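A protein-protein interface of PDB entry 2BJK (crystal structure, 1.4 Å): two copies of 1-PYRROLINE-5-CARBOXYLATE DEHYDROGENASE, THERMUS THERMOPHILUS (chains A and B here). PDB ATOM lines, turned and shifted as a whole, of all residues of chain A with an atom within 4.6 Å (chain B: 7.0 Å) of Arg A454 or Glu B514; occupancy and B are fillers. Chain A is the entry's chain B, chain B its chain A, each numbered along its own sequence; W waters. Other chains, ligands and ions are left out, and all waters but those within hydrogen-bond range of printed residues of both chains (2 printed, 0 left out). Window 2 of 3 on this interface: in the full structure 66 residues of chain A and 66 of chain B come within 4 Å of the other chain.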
ATOM      1  N   ARG A 452      -7.138  29.386  17.756  1.00  0.00           N
ATOM      2  CA  ARG A 452      -7.466  29.793  16.395  1.00  0.00           C
ATOM      3  C   ARG A 452      -6.415  29.216  15.449  1.00  0.00           C
ATOM      4  O   ARG A 452      -6.589  29.244  14.231  1.00  0.00           O
ATOM      5  CB  ARG A 452      -7.461  31.315  16.245  1.00  0.00           C
ATOM      6  CG  ARG A 452      -8.644  32.060  16.841  1.00  0.00           C
ATOM      7  CD  ARG A 452      -8.614  33.499  16.331  1.00  0.00           C
ATOM      8  NE  ARG A 452      -9.730  34.318  16.795  1.00  0.00           N
ATOM      9  CZ  ARG A 452      -9.738  35.016  17.927  1.00  0.00           C
ATOM     10  NH1 ARG A 452     -10.806  35.731  18.258  1.00  0.00           N
ATOM     11  NH2 ARG A 452      -8.679  35.010  18.724  1.00  0.00           N
ATOM     12  N   LYS A 453      -5.328  28.690  16.003  1.00  0.00           N
ATOM     13  CA  LYS A 453      -4.259  28.143  15.172  1.00  0.00           C
ATOM     14  C   LYS A 453      -4.619  26.762  14.646  1.00  0.00           C
ATOM     15  O   LYS A 453      -4.699  25.798  15.406  1.00  0.00           O
ATOM     16  CB  LYS A 453      -2.947  28.089  15.962  1.00  0.00           C
ATOM     17  CG  LYS A 453      -1.739  27.737  15.109  1.00  0.00           C
ATOM     18  CD  LYS A 453      -0.439  27.947  15.867  1.00  0.00           C
ATOM     19  CE  LYS A 453       0.757  27.567  15.013  1.00  0.00           C
ATOM     20  NZ  LYS A 453       0.777  28.334  13.737  1.00  0.00           N
ATOM     21  N   ARG A 454      -4.828  26.673  13.334  1.00  0.00           N
ATOM     22  CA  ARG A 454      -5.208  25.410  12.707  1.00  0.00           C
ATOM     23  C   ARG A 454      -4.262  24.264  13.040  1.00  0.00           C
ATOM     24  O   ARG A 454      -4.699  23.146  13.314  1.00  0.00           O
ATOM     25  CB  ARG A 454      -5.274  25.561  11.182  1.00  0.00           C
ATOM     26  CG  ARG A 454      -6.153  26.699  10.675  1.00  0.00           C
ATOM     27  CD  ARG A 454      -7.533  26.690  11.314  1.00  0.00           C
ATOM     28  NE  ARG A 454      -8.240  25.424  11.145  1.00  0.00           N
ATOM     29  CZ  ARG A 454      -9.420  25.161  11.700  1.00  0.00           C
ATOM     30  NH1 ARG A 454     -10.004  23.988  11.506  1.00  0.00           N
ATOM     31  NH2 ARG A 454     -10.018  26.077  12.450  1.00  0.00           N
ATOM     32  N   GLU A 455      -2.965  24.543  13.015  1.00  0.00           N
ATOM     33  CA  GLU A 455      -1.968  23.521  13.289  1.00  0.00           C
ATOM     34  C   GLU A 455      -2.073  22.942  14.696  1.00  0.00           C
ATOM     35  O   GLU A 455      -1.770  21.769  14.913  1.00  0.00           O
ATOM     36  CB  GLU A 455      -0.563  24.082  13.039  1.00  0.00           C
ATOM     37  CG  GLU A 455      -0.284  24.435  11.573  1.00  0.00           C
ATOM     38  CD  GLU A 455      -0.769  25.822  11.165  1.00  0.00           C
ATOM     39  OE1 GLU A 455      -1.501  26.474  11.938  1.00  0.00           O
ATOM     40  OE2 GLU A 455      -0.416  26.266  10.051  1.00  0.00           O
ATOM     41  N   HIS A 456      -2.500  23.757  15.654  1.00  0.00           N
ATOM     42  CA  HIS A 456      -2.644  23.273  17.020  1.00  0.00           C
ATOM     43  C   HIS A 456      -3.879  22.387  17.127  1.00  0.00           C
ATOM     44  O   HIS A 456      -3.845  21.342  17.771  1.00  0.00           O
ATOM     45  CB  HIS A 456      -2.741  24.443  18.004  1.00  0.00           C
ATOM     46  CG  HIS A 456      -1.431  25.123  18.262  1.00  0.00           C
ATOM     47  ND1 HIS A 456      -1.294  26.156  19.165  1.00  0.00           N
ATOM     48  CD2 HIS A 456      -0.196  24.904  17.751  1.00  0.00           C
ATOM     49  CE1 HIS A 456      -0.031  26.542  19.201  1.00  0.00           C
ATOM     50  NE2 HIS A 456       0.657  25.798  18.353  1.00  0.00           N
ATOM     51  N   LEU A 457      -4.966  22.799  16.479  1.00  0.00           N
ATOM     52  CA  LEU A 457      -6.190  22.013  16.510  1.00  0.00           C
ATOM     53  C   LEU A 457      -5.986  20.653  15.850  1.00  0.00           C
ATOM     54  O   LEU A 457      -6.356  19.625  16.415  1.00  0.00           O
ATOM     55  CB  LEU A 457      -7.329  22.760  15.807  1.00  0.00           C
ATOM     56  CG  LEU A 457      -7.798  24.064  16.464  1.00  0.00           C
ATOM     57  CD1 LEU A 457      -8.967  24.640  15.677  1.00  0.00           C
ATOM     58  CD2 LEU A 457      -8.213  23.803  17.907  1.00  0.00           C
ATOM     59  N   GLU A 458      -5.390  20.636  14.663  1.00  0.00           N
ATOM     60  CA  GLU A 458      -5.189  19.364  13.978  1.00  0.00           C
ATOM     61  C   GLU A 458      -4.164  18.489  14.709  1.00  0.00           C
ATOM     62  O   GLU A 458      -4.233  17.264  14.662  1.00  0.00           O
ATOM     63  CB  GLU A 458      -4.803  19.607  12.514  1.00  0.00           C
ATOM     64  CG  GLU A 458      -5.844  20.442  11.731  1.00  0.00           C
ATOM     65  CD  GLU A 458      -7.259  19.850  11.731  1.00  0.00           C
ATOM     66  OE1 GLU A 458      -8.193  20.531  11.242  1.00  0.00           O
ATOM     67  OE2 GLU A 458      -7.450  18.713  12.212  1.00  0.00           O
ATOM     68  N   ARG A 461      -6.111  16.941  17.400  1.00  0.00           N
ATOM     69  CA  ARG A 461      -7.008  15.944  16.828  1.00  0.00           C
ATOM     70  C   ARG A 461      -6.306  14.592  16.792  1.00  0.00           C
ATOM     71  O   ARG A 461      -6.929  13.550  16.986  1.00  0.00           O
ATOM     72  CB  ARG A 461      -7.419  16.356  15.410  1.00  0.00           C
ATOM     73  CG  ARG A 461      -8.350  15.370  14.701  1.00  0.00           C
ATOM     74  CD  ARG A 461      -8.762  15.885  13.319  1.00  0.00           C
ATOM     75  NE  ARG A 461      -9.472  17.156  13.422  1.00  0.00           N
ATOM     76  CZ  ARG A 461     -10.791  17.279  13.552  1.00  0.00           C
ATOM     77  NH1 ARG A 461     -11.573  16.207  13.578  1.00  0.00           N
ATOM     78  NH2 ARG A 461     -11.326  18.481  13.711  1.00  0.00           N
ATOM     79  N   PHE A 471     -13.381  21.308  19.975  1.00  0.00           N
ATOM     80  CA  PHE A 471     -12.610  22.507  19.679  1.00  0.00           C
ATOM     81  C   PHE A 471     -13.480  23.755  19.669  1.00  0.00           C
ATOM     82  O   PHE A 471     -14.499  23.816  18.978  1.00  0.00           O
ATOM     83  CB  PHE A 471     -11.914  22.385  18.319  1.00  0.00           C
ATOM     84  CG  PHE A 471     -10.934  21.251  18.223  1.00  0.00           C
ATOM     85  CD1 PHE A 471     -10.258  20.784  19.346  1.00  0.00           C
ATOM     86  CD2 PHE A 471     -10.657  20.673  16.988  1.00  0.00           C
ATOM     87  CE1 PHE A 471      -9.318  19.759  19.235  1.00  0.00           C
ATOM     88  CE2 PHE A 471      -9.722  19.651  16.869  1.00  0.00           C
ATOM     89  CZ  PHE A 471      -9.051  19.192  17.996  1.00  0.00           C
ATOM     90  N   GLY B 164     -23.414  24.315  12.320  1.00  0.00           N
ATOM     91  CA  GLY B 164     -22.239  25.087  12.695  1.00  0.00           C
ATOM     92  C   GLY B 164     -21.049  24.323  13.237  1.00  0.00           C
ATOM     93  O   GLY B 164     -20.127  24.923  13.794  1.00  0.00           O
ATOM     94  N   GLU B 165     -21.053  23.008  13.056  1.00  0.00           N
ATOM     95  CA  GLU B 165     -19.978  22.166  13.562  1.00  0.00           C
ATOM     96  C   GLU B 165     -19.544  21.077  12.603  1.00  0.00           C
ATOM     97  O   GLU B 165     -20.320  20.619  11.762  1.00  0.00           O
ATOM     98  CB  GLU B 165     -20.420  21.432  14.828  1.00  0.00           C
ATOM     99  CG  GLU B 165     -20.526  22.227  16.099  1.00  0.00           C
ATOM    100  CD  GLU B 165     -20.833  21.333  17.297  1.00  0.00           C
ATOM    101  OE1 GLU B 165     -20.782  21.839  18.433  1.00  0.00           O
ATOM    102  OE2 GLU B 165     -21.128  20.127  17.104  1.00  0.00           O
ATOM    103  N   ASP B 166     -18.294  20.660  12.758  1.00  0.00           N
ATOM    104  CA  ASP B 166     -17.776  19.529  12.008  1.00  0.00           C
ATOM    105  C   ASP B 166     -17.665  18.455  13.086  1.00  0.00           C
ATOM    106  O   ASP B 166     -17.066  18.683  14.141  1.00  0.00           O
ATOM    107  CB  ASP B 166     -16.390  19.802  11.420  1.00  0.00           C
ATOM    108  CG  ASP B 166     -15.859  18.619  10.621  1.00  0.00           C
ATOM    109  OD1 ASP B 166     -14.879  17.971  11.056  1.00  0.00           O
ATOM    110  OD2 ASP B 166     -16.434  18.332   9.550  1.00  0.00           O
ATOM    111  N   ASN B 167     -18.278  17.302  12.847  1.00  0.00           N
ATOM    112  CA  ASN B 167     -18.216  16.201  13.797  1.00  0.00           C
ATOM    113  C   ASN B 167     -17.647  15.020  13.062  1.00  0.00           C
ATOM    114  O   ASN B 167     -18.260  14.491  12.141  1.00  0.00           O
ATOM    115  CB  ASN B 167     -19.601  15.915  14.356  1.00  0.00           C
ATOM    116  CG  ASN B 167     -19.971  16.887  15.445  1.00  0.00           C
ATOM    117  OD1 ASN B 167     -19.479  16.781  16.567  1.00  0.00           O
ATOM    118  ND2 ASN B 167     -20.809  17.867  15.118  1.00  0.00           N
ATOM    119  N   GLU B 168     -16.453  14.625  13.478  1.00  0.00           N
ATOM    120  CA  GLU B 168     -15.724  13.554  12.832  1.00  0.00           C
ATOM    121  C   GLU B 168     -15.321  12.452  13.789  1.00  0.00           C
ATOM    122  O   GLU B 168     -14.602  12.694  14.757  1.00  0.00           O
ATOM    123  CB  GLU B 168     -14.474  14.157  12.197  1.00  0.00           C
ATOM    124  CG  GLU B 168     -13.644  13.235  11.347  1.00  0.00           C
ATOM    125  CD  GLU B 168     -12.418  13.941  10.827  1.00  0.00           C
ATOM    126  OE1 GLU B 168     -11.427  14.045  11.582  1.00  0.00           O
ATOM    127  OE2 GLU B 168     -12.457  14.420   9.673  1.00  0.00           O
ATOM    128  N   VAL B 512     -14.297  13.766  17.325  1.00  0.00           N
ATOM    129  CA  VAL B 512     -13.770  15.121  17.427  1.00  0.00           C
ATOM    130  C   VAL B 512     -14.710  16.126  16.789  1.00  0.00           C
ATOM    131  O   VAL B 512     -15.071  16.006  15.621  1.00  0.00           O
ATOM    132  CB  VAL B 512     -12.392  15.211  16.752  1.00  0.00           C
ATOM    133  CG1 VAL B 512     -11.795  16.588  16.963  1.00  0.00           C
ATOM    134  CG2 VAL B 512     -11.469  14.132  17.315  1.00  0.00           C
ATOM    135  N   ALA B 513     -15.094  17.125  17.572  1.00  0.00           N
ATOM    136  CA  ALA B 513     -16.007  18.157  17.113  1.00  0.00           C
ATOM    137  C   ALA B 513     -15.346  19.522  17.100  1.00  0.00           C
ATOM    138  O   ALA B 513     -14.604  19.870  18.022  1.00  0.00           O
ATOM    139  CB  ALA B 513     -17.229  18.203  18.025  1.00  0.00           C
ATOM    140  N   GLU B 514     -15.586  20.284  16.039  1.00  0.00           N
ATOM    141  CA  GLU B 514     -15.077  21.644  15.975  1.00  0.00           C
ATOM    142  C   GLU B 514     -16.244  22.572  15.709  1.00  0.00           C
ATOM    143  O   GLU B 514     -16.968  22.412  14.723  1.00  0.00           O
ATOM    144  CB  GLU B 514     -14.029  21.867  14.877  1.00  0.00           C
ATOM    145  CG  GLU B 514     -13.604  23.346  14.856  1.00  0.00           C
ATOM    146  CD  GLU B 514     -12.532  23.706  13.850  1.00  0.00           C
ATOM    147  OE1 GLU B 514     -11.958  22.800  13.215  1.00  0.00           O
ATOM    148  OE2 GLU B 514     -12.261  24.919  13.711  1.00  0.00           O
ATOM    149  N   ARG B 515     -16.442  23.527  16.609  1.00  0.00           N
ATOM    150  CA  ARG B 515     -17.496  24.521  16.452  1.00  0.00           C
ATOM    151  C   ARG B 515     -16.831  25.695  15.742  1.00  0.00           C
ATOM    152  O   ARG B 515     -15.890  26.296  16.264  1.00  0.00           O
ATOM    153  CB  ARG B 515     -18.020  24.967  17.816  1.00  0.00           C
ATOM    154  CG  ARG B 515     -19.120  26.018  17.748  1.00  0.00           C
ATOM    155  CD  ARG B 515     -20.439  25.426  17.291  1.00  0.00           C
ATOM    156  NE  ARG B 515     -20.967  24.452  18.245  1.00  0.00           N
ATOM    157  CZ  ARG B 515     -21.373  24.742  19.479  1.00  0.00           C
ATOM    158  NH1 ARG B 515     -21.839  23.781  20.267  1.00  0.00           N
ATOM    159  NH2 ARG B 515     -21.323  25.990  19.927  1.00  0.00           N
ATOM    160  N   PHE B 516     -17.308  26.016  14.546  1.00  0.00           N
ATOM    161  CA  PHE B 516     -16.713  27.099  13.770  1.00  0.00           C
ATOM    162  C   PHE B 516     -17.075  28.505  14.228  1.00  0.00           C
ATOM    163  O   PHE B 516     -16.258  29.418  13.974  1.00  0.00           O
ATOM    164  CB  PHE B 516     -17.057  26.918  12.293  1.00  0.00           C
ATOM    165  CG  PHE B 516     -16.547  25.628  11.721  1.00  0.00           C
ATOM    166  CD1 PHE B 516     -17.432  24.643  11.293  1.00  0.00           C
ATOM    167  CD2 PHE B 516     -15.179  25.386  11.633  1.00  0.00           C
ATOM    168  CE1 PHE B 516     -16.959  23.435  10.790  1.00  0.00           C
ATOM    169  CE2 PHE B 516     -14.697  24.181  11.131  1.00  0.00           C
ATOM    170  CZ  PHE B 516     -15.589  23.204  10.708  1.00  0.00           C
ATOM    171  OXT PHE B 516     -18.161  28.684  14.816  1.00  0.00           O
HETATM  172  O   HOH W   1     -14.020  17.756  13.619  1.00  0.00           O
HETATM  173  O   HOH W   2      -9.885  20.995  13.588  1.00  0.00           O
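No position is printed for both chains.
CD1 of Leu A457 touches OE2 of Glu B514 (3.8 Å).
Arg A461 touches Val B512.
Val B512 touches Phe A471.
Phe A471 touches Glu B514 (O to CA, 3.8 Å).
Of chain B, only Glu B514 (2.8 Å) comes within 4 Å of Arg A454.
Printed residues of chain A within 4 Å of Glu B514: Arg A454 (2.8 Å), Leu A457 (3.8 Å) and Phe A471 (3.8 Å).
Of the printed residues of chain A, Val B512 touches Arg A461 (3.4 Å) and Phe A471 (3.7 Å).
Of the printed residues of chain B, Leu A457 touches Glu B514.
Of the printed residues of chain A, Arg B515 touches Phe A471 (3.1 Å).
Of the printed residues of chain B, Phe A471 touches Val B512 (3.7 Å), Ala B513 (2.7 Å), Glu B514 (3.8 Å) and Arg B515 (3.1 Å).
Of the printed residues of chain B, Arg A461 touches Glu B168 and Val B512.
The nearest residue of chain B that does not touch Arg A454 is Phe B516 (4.7 Å).
Along chain B the printed residues that touch a printed residue of chain A span positions 168 to 515.
Among the printed residues, 8 pairs touch across the chains.
Among the printed residues, Asp or Glu carboxylates within 4 Å of a Lys or Arg side-chain nitrogen of the other chain: Arg A454 with Glu B514 (2.8 Å) and Arg A461 with Glu B168 (2.9 Å).
Water W1 lies within hydrogen-bond range of the side-chain carboxylate (OD1) of Asp B166 (2.7 Å), the guanidinium group (NH2) of Arg A461 (2.8 Å) and the backbone carbonyl oxygen (O) of Val B512 (2.9 Å).
Water W2 lies within hydrogen-bond range of OE1 of Glu B514 (2.8 Å), NH2 of Arg A461 (2.9 Å) and OE1 of Glu A458 (2.9 Å).
The backbone carbonyl oxygen (O) of Asp B166 sits at hydrogen-bond distance from the backbone NH (N) of Glu B514, at 2.9 Å.
OE2 of Glu A458 is in salt-bridge range of NE of Arg A461 (2.8 Å).
The guanidinium group (NH1) of Arg A454 is in salt-bridge range of the side-chain carboxylate (OE1) of Glu A458, at 3.9 Å.
The guanidinium group (NE) of Arg B515 lies within salt-bridge range of the side-chain carboxylate (OE1) of Glu B165 (2.6 Å).
N of Val B512 lies within hydrogen-bond range of O of Glu B168.
The backbone NH (N) of Phe A471 lies within hydrogen-bond range of the backbone carbonyl oxygen (O) of Ala B513 (2.7 Å).
The guanidinium group (NH2) of Arg A454 lies within salt-bridge range of the side-chain carboxylate (OE2) of Glu B514.
The backbone carbonyl oxygen (O) of Phe A471 is in hydrogen-bond range of the backbone NH (N) of Arg B515 (3.1 Å).
OE1 of Glu B168 is in salt-bridge range of NH1 of Arg A461.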
